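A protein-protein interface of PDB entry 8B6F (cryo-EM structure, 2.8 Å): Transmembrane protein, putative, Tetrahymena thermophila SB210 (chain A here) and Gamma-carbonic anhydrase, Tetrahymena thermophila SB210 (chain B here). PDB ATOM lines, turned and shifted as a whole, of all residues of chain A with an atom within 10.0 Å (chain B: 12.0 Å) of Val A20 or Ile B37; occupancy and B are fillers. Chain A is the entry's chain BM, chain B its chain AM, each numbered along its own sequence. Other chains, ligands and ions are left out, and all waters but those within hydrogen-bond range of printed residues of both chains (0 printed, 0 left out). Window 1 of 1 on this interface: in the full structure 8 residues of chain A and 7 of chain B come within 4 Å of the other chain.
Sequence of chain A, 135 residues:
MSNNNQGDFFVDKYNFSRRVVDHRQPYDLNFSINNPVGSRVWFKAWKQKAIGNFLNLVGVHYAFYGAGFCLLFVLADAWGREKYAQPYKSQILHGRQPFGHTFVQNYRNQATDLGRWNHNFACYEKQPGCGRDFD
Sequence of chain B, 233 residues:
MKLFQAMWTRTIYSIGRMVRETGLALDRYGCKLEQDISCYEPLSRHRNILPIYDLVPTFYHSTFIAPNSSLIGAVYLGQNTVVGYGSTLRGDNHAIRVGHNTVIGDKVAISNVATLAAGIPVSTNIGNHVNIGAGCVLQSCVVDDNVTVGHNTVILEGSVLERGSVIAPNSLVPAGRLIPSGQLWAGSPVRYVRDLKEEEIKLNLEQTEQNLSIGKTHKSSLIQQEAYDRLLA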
ATOM      1  N   ASN A  15     -24.096  -5.015  11.381  1.00  0.00           N
ATOM      2  CA  ASN A  15     -25.376  -4.618  10.800  1.00  0.00           C
ATOM      3  C   ASN A  15     -25.636  -5.512   9.594  1.00  0.00           C
ATOM      4  O   ASN A  15     -25.034  -5.334   8.533  1.00  0.00           O
ATOM      5  CB  ASN A  15     -25.342  -3.141  10.420  1.00  0.00           C
ATOM      6  CG  ASN A  15     -26.582  -2.698   9.675  1.00  0.00           C
ATOM      7  OD1 ASN A  15     -27.580  -3.410   9.623  1.00  0.00           O
ATOM      8  ND2 ASN A  15     -26.522  -1.509   9.092  1.00  0.00           N
ATOM      9  N   SER A  17     -28.034  -5.608   7.620  1.00  0.00           N
ATOM     10  CA  SER A  17     -28.660  -4.908   6.506  1.00  0.00           C
ATOM     11  C   SER A  17     -27.799  -3.754   6.004  1.00  0.00           C
ATOM     12  O   SER A  17     -28.301  -2.872   5.302  1.00  0.00           O
ATOM     13  CB  SER A  17     -30.046  -4.405   6.905  1.00  0.00           C
ATOM     14  OG  SER A  17     -29.962  -3.472   7.966  1.00  0.00           O
ATOM     15  N   ARG A  18     -26.515  -3.741   6.355  1.00  0.00           N
ATOM     16  CA  ARG A  18     -25.624  -2.689   5.890  1.00  0.00           C
ATOM     17  C   ARG A  18     -25.622  -2.641   4.369  1.00  0.00           C
ATOM     18  O   ARG A  18     -25.576  -3.675   3.699  1.00  0.00           O
ATOM     19  CB  ARG A  18     -24.205  -2.933   6.407  1.00  0.00           C
ATOM     20  CG  ARG A  18     -23.234  -1.794   6.142  1.00  0.00           C
ATOM     21  CD  ARG A  18     -23.471  -0.637   7.092  1.00  0.00           C
ATOM     22  NE  ARG A  18     -22.574   0.482   6.828  1.00  0.00           N
ATOM     23  CZ  ARG A  18     -22.852   1.502   6.028  1.00  0.00           C
ATOM     24  NH1 ARG A  18     -24.002   1.582   5.381  1.00  0.00           N
ATOM     25  NH2 ARG A  18     -21.953   2.470   5.875  1.00  0.00           N
ATOM     26  N   ARG A  19     -25.677  -1.429   3.820  1.00  0.00           N
ATOM     27  CA  ARG A  19     -25.737  -1.274   2.373  1.00  0.00           C
ATOM     28  C   ARG A  19     -25.356   0.147   1.994  1.00  0.00           C
ATOM     29  O   ARG A  19     -25.935   1.105   2.513  1.00  0.00           O
ATOM     30  CB  ARG A  19     -27.138  -1.610   1.852  1.00  0.00           C
ATOM     31  CG  ARG A  19     -27.333  -1.314   0.376  1.00  0.00           C
ATOM     32  CD  ARG A  19     -28.625  -1.918  -0.149  1.00  0.00           C
ATOM     33  NE  ARG A  19     -28.854  -1.566  -1.545  1.00  0.00           N
ATOM     34  CZ  ARG A  19     -28.224  -2.119  -2.573  1.00  0.00           C
ATOM     35  NH1 ARG A  19     -27.301  -3.050  -2.400  1.00  0.00           N
ATOM     36  NH2 ARG A  19     -28.523  -1.722  -3.806  1.00  0.00           N
ATOM     37  N   VAL A  20     -24.385   0.274   1.093  1.00  0.00           N
ATOM     38  CA  VAL A  20     -24.021   1.550   0.487  1.00  0.00           C
ATOM     39  C   VAL A  20     -24.099   1.369  -1.022  1.00  0.00           C
ATOM     40  O   VAL A  20     -23.400   0.517  -1.582  1.00  0.00           O
ATOM     41  CB  VAL A  20     -22.618   2.018   0.909  1.00  0.00           C
ATOM     42  CG1 VAL A  20     -22.309   3.382   0.312  1.00  0.00           C
ATOM     43  CG2 VAL A  20     -22.501   2.057   2.420  1.00  0.00           C
ATOM     44  N   VAL A  21     -24.942   2.165  -1.678  1.00  0.00           N
ATOM     45  CA  VAL A  21     -25.171   1.996  -3.106  1.00  0.00           C
ATOM     46  C   VAL A  21     -23.951   2.463  -3.885  1.00  0.00           C
ATOM     47  O   VAL A  21     -23.339   3.492  -3.568  1.00  0.00           O
ATOM     48  CB  VAL A  21     -26.436   2.755  -3.540  1.00  0.00           C
ATOM     49  CG1 VAL A  21     -26.598   2.726  -5.054  1.00  0.00           C
ATOM     50  CG2 VAL A  21     -27.657   2.160  -2.870  1.00  0.00           C
ATOM     51  N   ASP A  22     -23.594   1.704  -4.918  1.00  0.00           N
ATOM     52  CA  ASP A  22     -22.440   2.023  -5.751  1.00  0.00           C
ATOM     53  C   ASP A  22     -22.784   3.194  -6.664  1.00  0.00           C
ATOM     54  O   ASP A  22     -23.577   3.051  -7.600  1.00  0.00           O
ATOM     55  CB  ASP A  22     -22.033   0.797  -6.562  1.00  0.00           C
ATOM     56  CG  ASP A  22     -20.733   0.996  -7.307  1.00  0.00           C
ATOM     57  OD1 ASP A  22     -20.070   2.028  -7.083  1.00  0.00           O
ATOM     58  OD2 ASP A  22     -20.375   0.117  -8.118  1.00  0.00           O
ATOM     59  N   HIS A  23     -22.187   4.354  -6.394  1.00  0.00           N
ATOM     60  CA  HIS A  23     -22.445   5.548  -7.188  1.00  0.00           C
ATOM     61  C   HIS A  23     -21.765   5.512  -8.550  1.00  0.00           C
ATOM     62  O   HIS A  23     -22.052   6.374  -9.385  1.00  0.00           O
ATOM     63  CB  HIS A  23     -21.984   6.791  -6.428  1.00  0.00           C
ATOM     64  CG  HIS A  23     -20.502   6.857  -6.226  1.00  0.00           C
ATOM     65  ND1 HIS A  23     -19.834   6.049  -5.331  1.00  0.00           N
ATOM     66  CD2 HIS A  23     -19.559   7.637  -6.804  1.00  0.00           C
ATOM     67  CE1 HIS A  23     -18.545   6.327  -5.367  1.00  0.00           C
ATOM     68  NE2 HIS A  23     -18.350   7.288  -6.252  1.00  0.00           N
ATOM     69  N   ARG A  24     -20.867   4.559  -8.787  1.00  0.00           N
ATOM     70  CA  ARG A  24     -20.149   4.460 -10.055  1.00  0.00           C
ATOM     71  C   ARG A  24     -20.974   3.593 -10.995  1.00  0.00           C
ATOM     72  O   ARG A  24     -20.985   2.367 -10.877  1.00  0.00           O
ATOM     73  CB  ARG A  24     -18.757   3.880  -9.840  1.00  0.00           C
ATOM     74  CG  ARG A  24     -17.928   4.632  -8.810  1.00  0.00           C
ATOM     75  CD  ARG A  24     -16.691   3.849  -8.410  1.00  0.00           C
ATOM     76  NE  ARG A  24     -17.034   2.550  -7.844  1.00  0.00           N
ATOM     77  CZ  ARG A  24     -16.157   1.695  -7.338  1.00  0.00           C
ATOM     78  NH1 ARG A  24     -14.865   1.972  -7.296  1.00  0.00           N
ATOM     79  NH2 ARG A  24     -16.589   0.533  -6.857  1.00  0.00           N
ATOM     80  N   GLN A  25     -21.662   4.230 -11.936  1.00  0.00           N
ATOM     81  CA  GLN A  25     -22.487   3.534 -12.908  1.00  0.00           C
ATOM     82  C   GLN A  25     -22.112   3.988 -14.310  1.00  0.00           C
ATOM     83  O   GLN A  25     -21.731   5.144 -14.509  1.00  0.00           O
ATOM     84  CB  GLN A  25     -23.978   3.807 -12.667  1.00  0.00           C
ATOM     85  CG  GLN A  25     -24.482   3.361 -11.307  1.00  0.00           C
ATOM     86  CD  GLN A  25     -24.484   1.854 -11.151  1.00  0.00           C
ATOM     87  OE1 GLN A  25     -24.190   1.120 -12.092  1.00  0.00           O
ATOM     88  NE2 GLN A  25     -24.819   1.386  -9.955  1.00  0.00           N
ATOM     89  N   LEU B  24     -15.463 -12.889   6.074  1.00  0.00           N
ATOM     90  CA  LEU B  24     -15.233 -11.549   5.544  1.00  0.00           C
ATOM     91  C   LEU B  24     -15.044 -11.578   4.033  1.00  0.00           C
ATOM     92  O   LEU B  24     -15.525 -10.687   3.325  1.00  0.00           O
ATOM     93  CB  LEU B  24     -14.026 -10.916   6.235  1.00  0.00           C
ATOM     94  CG  LEU B  24     -14.194 -10.713   7.744  1.00  0.00           C
ATOM     95  CD1 LEU B  24     -12.886 -10.310   8.398  1.00  0.00           C
ATOM     96  CD2 LEU B  24     -15.263  -9.668   8.023  1.00  0.00           C
ATOM     97  N   ASP B  27     -18.421 -11.945   2.457  1.00  0.00           N
ATOM     98  CA  ASP B  27     -19.149 -10.684   2.501  1.00  0.00           C
ATOM     99  C   ASP B  27     -18.655  -9.732   1.419  1.00  0.00           C
ATOM    100  O   ASP B  27     -19.458  -9.064   0.758  1.00  0.00           O
ATOM    101  CB  ASP B  27     -19.013 -10.051   3.885  1.00  0.00           C
ATOM    102  CG  ASP B  27     -19.987  -8.912   4.102  1.00  0.00           C
ATOM    103  OD1 ASP B  27     -20.147  -8.077   3.190  1.00  0.00           O
ATOM    104  OD2 ASP B  27     -20.603  -8.855   5.185  1.00  0.00           O
ATOM    105  N   ARG B  28     -17.337  -9.648   1.229  1.00  0.00           N
ATOM    106  CA  ARG B  28     -16.800  -8.790   0.179  1.00  0.00           C
ATOM    107  C   ARG B  28     -17.258  -9.254  -1.197  1.00  0.00           C
ATOM    108  O   ARG B  28     -17.622  -8.434  -2.047  1.00  0.00           O
ATOM    109  CB  ARG B  28     -15.275  -8.755   0.245  1.00  0.00           C
ATOM    110  CG  ARG B  28     -14.726  -7.754   1.242  1.00  0.00           C
ATOM    111  CD  ARG B  28     -13.368  -7.238   0.796  1.00  0.00           C
ATOM    112  NE  ARG B  28     -12.920  -6.118   1.614  1.00  0.00           N
ATOM    113  CZ  ARG B  28     -11.909  -5.319   1.300  1.00  0.00           C
ATOM    114  NH1 ARG B  28     -11.215  -5.488   0.186  1.00  0.00           N
ATOM    115  NH2 ARG B  28     -11.591  -4.323   2.120  1.00  0.00           N
ATOM    116  N   TYR B  29     -17.246 -10.565  -1.437  1.00  0.00           N
ATOM    117  CA  TYR B  29     -17.689 -11.083  -2.726  1.00  0.00           C
ATOM    118  C   TYR B  29     -19.169 -10.796  -2.947  1.00  0.00           C
ATOM    119  O   TYR B  29     -19.586 -10.467  -4.063  1.00  0.00           O
ATOM    120  CB  TYR B  29     -17.409 -12.581  -2.816  1.00  0.00           C
ATOM    121  CG  TYR B  29     -17.779 -13.181  -4.151  1.00  0.00           C
ATOM    122  CD1 TYR B  29     -17.033 -12.903  -5.288  1.00  0.00           C
ATOM    123  CD2 TYR B  29     -18.866 -14.034  -4.272  1.00  0.00           C
ATOM    124  CE1 TYR B  29     -17.363 -13.451  -6.509  1.00  0.00           C
ATOM    125  CE2 TYR B  29     -19.205 -14.586  -5.488  1.00  0.00           C
ATOM    126  CZ  TYR B  29     -18.448 -14.292  -6.603  1.00  0.00           C
ATOM    127  OH  TYR B  29     -18.783 -14.844  -7.818  1.00  0.00           O
ATOM    128  N   GLY B  30     -19.975 -10.914  -1.893  1.00  0.00           N
ATOM    129  CA  GLY B  30     -21.380 -10.564  -2.007  1.00  0.00           C
ATOM    130  C   GLY B  30     -21.583  -9.098  -2.336  1.00  0.00           C
ATOM    131  O   GLY B  30     -22.442  -8.747  -3.146  1.00  0.00           O
ATOM    132  N   CYS B  31     -20.792  -8.223  -1.712  1.00  0.00           N
ATOM    133  CA  CYS B  31     -20.847  -6.804  -2.051  1.00  0.00           C
ATOM    134  C   CYS B  31     -20.496  -6.579  -3.516  1.00  0.00           C
ATOM    135  O   CYS B  31     -21.156  -5.796  -4.207  1.00  0.00           O
ATOM    136  CB  CYS B  31     -19.899  -6.011  -1.152  1.00  0.00           C
ATOM    137  SG  CYS B  31     -20.417  -5.896   0.570  1.00  0.00           S
ATOM    138  N   LYS B  32     -19.459  -7.259  -4.009  1.00  0.00           N
ATOM    139  CA  LYS B  32     -19.075  -7.115  -5.409  1.00  0.00           C
ATOM    140  C   LYS B  32     -20.208  -7.545  -6.329  1.00  0.00           C
ATOM    141  O   LYS B  32     -20.454  -6.913  -7.362  1.00  0.00           O
ATOM    142  CB  LYS B  32     -17.812  -7.927  -5.693  1.00  0.00           C
ATOM    143  CG  LYS B  32     -16.581  -7.427  -4.957  1.00  0.00           C
ATOM    144  CD  LYS B  32     -15.422  -8.404  -5.086  1.00  0.00           C
ATOM    145  CE  LYS B  32     -14.258  -7.999  -4.194  1.00  0.00           C
ATOM    146  NZ  LYS B  32     -13.161  -9.009  -4.224  1.00  0.00           N
ATOM    147  N   LEU B  33     -20.913  -8.619  -5.970  1.00  0.00           N
ATOM    148  CA  LEU B  33     -21.993  -9.113  -6.816  1.00  0.00           C
ATOM    149  C   LEU B  33     -23.213  -8.204  -6.731  1.00  0.00           C
ATOM    150  O   LEU B  33     -23.983  -8.112  -7.692  1.00  0.00           O
ATOM    151  CB  LEU B  33     -22.369 -10.537  -6.404  1.00  0.00           C
ATOM    152  CG  LEU B  33     -21.464 -11.689  -6.851  1.00  0.00           C
ATOM    153  CD1 LEU B  33     -22.080 -13.015  -6.445  1.00  0.00           C
ATOM    154  CD2 LEU B  33     -21.207 -11.675  -8.350  1.00  0.00           C
ATOM    155  N   GLU B  34     -23.399  -7.536  -5.598  1.00  0.00           N
ATOM    156  CA  GLU B  34     -24.569  -6.708  -5.335  1.00  0.00           C
ATOM    157  C   GLU B  34     -24.361  -5.252  -5.728  1.00  0.00           C
ATOM    158  O   GLU B  34     -25.272  -4.438  -5.541  1.00  0.00           O
ATOM    159  CB  GLU B  34     -24.922  -6.782  -3.847  1.00  0.00           C
ATOM    160  CG  GLU B  34     -26.401  -6.803  -3.538  1.00  0.00           C
ATOM    161  CD  GLU B  34     -26.665  -6.879  -2.049  1.00  0.00           C
ATOM    162  OE1 GLU B  34     -25.685  -6.917  -1.278  1.00  0.00           O
ATOM    163  OE2 GLU B  34     -27.847  -6.897  -1.648  1.00  0.00           O
ATOM    164  N   GLN B  35     -23.192  -4.905  -6.265  1.00  0.00           N
ATOM    165  CA  GLN B  35     -22.848  -3.519  -6.590  1.00  0.00           C
ATOM    166  C   GLN B  35     -22.952  -2.623  -5.356  1.00  0.00           C
ATOM    167  O   GLN B  35     -23.507  -1.524  -5.406  1.00  0.00           O
ATOM    168  CB  GLN B  35     -23.724  -2.995  -7.731  1.00  0.00           C
ATOM    169  CG  GLN B  35     -23.650  -3.866  -8.975  1.00  0.00           C
ATOM    170  CD  GLN B  35     -24.334  -3.245 -10.174  1.00  0.00           C
ATOM    171  OE1 GLN B  35     -25.033  -2.241 -10.058  1.00  0.00           O
ATOM    172  NE2 GLN B  35     -24.142  -3.853 -11.341  1.00  0.00           N
ATOM    173  N   ASP B  36     -22.433  -3.117  -4.237  1.00  0.00           N
ATOM    174  CA  ASP B  36     -22.439  -2.420  -2.957  1.00  0.00           C
ATOM    175  C   ASP B  36     -21.011  -2.005  -2.612  1.00  0.00           C
ATOM    176  O   ASP B  36     -20.090  -2.819  -2.713  1.00  0.00           O
ATOM    177  CB  ASP B  36     -23.034  -3.327  -1.879  1.00  0.00           C
ATOM    178  CG  ASP B  36     -23.194  -2.633  -0.550  1.00  0.00           C
ATOM    179  OD1 ASP B  36     -22.232  -1.996  -0.078  1.00  0.00           O
ATOM    180  OD2 ASP B  36     -24.295  -2.732   0.026  1.00  0.00           O
ATOM    181  N   ILE B  37     -20.825  -0.745  -2.211  1.00  0.00           N
ATOM    182  CA  ILE B  37     -19.493  -0.194  -1.951  1.00  0.00           C
ATOM    183  C   ILE B  37     -19.154  -0.160  -0.457  1.00  0.00           C
ATOM    184  O   ILE B  37     -18.143   0.430  -0.072  1.00  0.00           O
ATOM    185  CB  ILE B  37     -19.311   1.189  -2.597  1.00  0.00           C
ATOM    186  CG1 ILE B  37     -20.444   2.136  -2.218  1.00  0.00           C
ATOM    187  CG2 ILE B  37     -19.204   1.051  -4.111  1.00  0.00           C
ATOM    188  CD1 ILE B  37     -20.153   3.573  -2.583  1.00  0.00           C
ATOM    189  N   SER B  38     -19.980  -0.775   0.392  1.00  0.00           N
ATOM    190  CA  SER B  38     -19.826  -0.657   1.843  1.00  0.00           C
ATOM    191  C   SER B  38     -18.481  -1.210   2.313  1.00  0.00           C
ATOM    192  O   SER B  38     -17.832  -0.625   3.187  1.00  0.00           O
ATOM    193  CB  SER B  38     -20.980  -1.363   2.551  1.00  0.00           C
ATOM    194  OG  SER B  38     -20.973  -2.752   2.281  1.00  0.00           O
ATOM    195  N   CYS B  39     -18.051  -2.334   1.741  1.00  0.00           N
ATOM    196  CA  CYS B  39     -16.807  -2.990   2.144  1.00  0.00           C
ATOM    197  C   CYS B  39     -15.602  -2.095   1.880  1.00  0.00           C
ATOM    198  O   CYS B  39     -14.655  -2.063   2.674  1.00  0.00           O
ATOM    199  CB  CYS B  39     -16.655  -4.323   1.411  1.00  0.00           C
ATOM    200  SG  CYS B  39     -16.993  -4.249  -0.362  1.00  0.00           S
ATOM    201  N   TYR B  40     -15.623  -1.361   0.771  1.00  0.00           N
ATOM    202  CA  TYR B  40     -14.492  -0.556   0.323  1.00  0.00           C
ATOM    203  C   TYR B  40     -14.149   0.578   1.283  1.00  0.00           C
ATOM    204  O   TYR B  40     -13.013   1.059   1.260  1.00  0.00           O
ATOM    205  CB  TYR B  40     -14.785   0.025  -1.059  1.00  0.00           C
ATOM    206  CG  TYR B  40     -15.160  -1.012  -2.089  1.00  0.00           C
ATOM    207  CD1 TYR B  40     -14.580  -2.274  -2.079  1.00  0.00           C
ATOM    208  CD2 TYR B  40     -16.100  -0.730  -3.070  1.00  0.00           C
ATOM    209  CE1 TYR B  40     -14.925  -3.224  -3.017  1.00  0.00           C
ATOM    210  CE2 TYR B  40     -16.449  -1.672  -4.014  1.00  0.00           C
ATOM    211  CZ  TYR B  40     -15.860  -2.918  -3.983  1.00  0.00           C
ATOM    212  OH  TYR B  40     -16.209  -3.858  -4.925  1.00  0.00           O
ATOM    213  N   GLU B  41     -15.086   1.025   2.112  1.00  0.00           N
ATOM    214  CA  GLU B  41     -14.874   2.239   2.887  1.00  0.00           C
ATOM    215  C   GLU B  41     -13.633   2.138   3.763  1.00  0.00           C
ATOM    216  O   GLU B  41     -13.429   1.116   4.434  1.00  0.00           O
ATOM    217  CB  GLU B  41     -16.063   2.504   3.809  1.00  0.00           C
ATOM    218  CG  GLU B  41     -15.966   3.842   4.533  1.00  0.00           C
ATOM    219  CD  GLU B  41     -17.277   4.294   5.140  1.00  0.00           C
ATOM    220  OE1 GLU B  41     -18.270   3.543   5.051  1.00  0.00           O
ATOM    221  OE2 GLU B  41     -17.306   5.395   5.729  1.00  0.00           O
ATOM    222  N   PRO B  42     -12.787   3.178   3.794  1.00  0.00           N
ATOM    223  CA  PRO B  42     -11.613   3.152   4.667  1.00  0.00           C
ATOM    224  C   PRO B  42     -11.950   3.823   5.981  1.00  0.00           C
ATOM    225  O   PRO B  42     -12.277   5.013   6.025  1.00  0.00           O
ATOM    226  CB  PRO B  42     -10.582   3.950   3.869  1.00  0.00           C
ATOM    227  CG  PRO B  42     -11.418   4.990   3.174  1.00  0.00           C
ATOM    228  CD  PRO B  42     -12.803   4.399   2.967  1.00  0.00           C
ATOM    229  N   LEU B  43     -11.861   3.059   7.056  1.00  0.00           N
ATOM    230  CA  LEU B  43     -12.187   3.533   8.384  1.00  0.00           C
ATOM    231  C   LEU B  43     -11.026   3.167   9.289  1.00  0.00           C
ATOM    232  O   LEU B  43     -10.328   2.181   9.043  1.00  0.00           O
ATOM    233  CB  LEU B  43     -13.487   2.875   8.856  1.00  0.00           C
ATOM    234  CG  LEU B  43     -14.771   3.518   8.328  1.00  0.00           C
ATOM    235  CD1 LEU B  43     -15.868   2.474   8.211  1.00  0.00           C
ATOM    236  CD2 LEU B  43     -15.232   4.652   9.217  1.00  0.00           C
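O of Val A20 is in hydrogen-bond range of N of Ile B37 (2.9 Å). NH2 of Arg A18 is in salt-bridge range of OE1 of Glu B41, 3.9 Å away. OE2 of Glu B34 is in salt-bridge range of NH1 of Arg A19, 3.96 Å away. O of Gln B35 sits close to N of Asp A22, at 3.3 Å. The side-chain carboxylate of Asp B36 lies within salt-bridge range of the guanidinium group of Arg A19, 3.9 Å away. The side-chain carboxylate of Asp B36 sits at hydrogen-bond distance from the backbone NH of Val A20 (3.2 Å).
SG of Cys B31 is in hydrogen-bond range of OG of Ser B38 (3.6 Å). The side-chain amide oxygen (OD1) of Asn A15 is in hydrogen-bond range of the backbone NH (N) of Arg A18. OD1 of Asp A22 lies within salt-bridge range of NE of Arg A24. The backbone carbonyl oxygen (O) of Asp A22 sits at hydrogen-bond distance from the side-chain amide nitrogen (NE2) of Gln A25, 3.1 Å away. OD1 of Asp B36 is in hydrogen-bond range of N of Ser B38, at 2.6 Å. The backbone carbonyl oxygen (O) of Cys B31 is in hydrogen-bond range of the backbone NH (N) of Asp B36, at 3.0 Å.
Ser B38 touches Val A20 (CB to CG2, 3.7 Å). Val A21 touches Ile B37 (O to CD1, 3.3 Å). Asp A22 touches Ile B37. CD1 of Ile B37 touches ND1 of His A23, at 3.7 Å. Ile B37 touches Arg A24. Arg A24 touches Tyr B40. NE2 of Gln A25 touches OE1 of Gln B35, 3.6 Å away.
Of the printed residues of chain B, Arg A18 touches Glu B41 (3.9 Å). Of chain B, only Asp B36 (3.2 Å), Ile B37 (2.9 Å) and Ser B38 (3.7 Å) come within 4 Å of Val A20. Asp A22 touches just these residues of chain B: Gln B35 (3.0 Å) and Ile B37 (3.2 Å). His A23 touches just one residue of chain B: Ile B37. Of the printed residues of chain B, Gln A25 touches Gln B35 (3.6 Å). Arg B28 touches none of the printed residues of chain A. Of the printed residues of chain A, Gln B35 touches Asp A22 and Gln A25. Printed residues of chain A within 4 Å of Asp B36: Arg A19 (3.1 Å) and Val A20 (3.2 Å). Ile B37 touches five residues of chain A. Ser B38 touches one residue of chain A. Tyr B40 touches one residue of chain A. Leu B43 touches none of the printed residues of chain A. The nearest residue of chain B that does not touch Val A20 is Gln B35 (4.3 Å). The nearest residue of chain A that does not touch Ile B37 is Arg A19 (6.2 Å). The nearest printed residue of chain A that does not touch Glu B34 is Arg A18 (5.9 Å).
Of the 10 printed residues of chain A, 8 touch a printed residue of chain B. Printed residues of chain A that touch a printed residue of chain B: Arg A18, Arg A19, Val A20, Val A21, Asp A22, His A23, Arg A24 and Gln A25. Hydrophobic or aromatic side chains of chain A that line the printed part of chain B: Val A20 and His A23. Hydrophobic or aromatic side chains of chain B within 4 Å of the printed part of chain A: Ile B37 and Tyr B40. Among the printed residues, 13 pairs touch across the chains. Among the printed residues, Asp or Glu carboxylates within 4 Å of a Lys or Arg side-chain nitrogen of the other chain: Arg A18 with Glu B41, Arg A19 with Glu B34 and Arg A19 with Asp B36.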
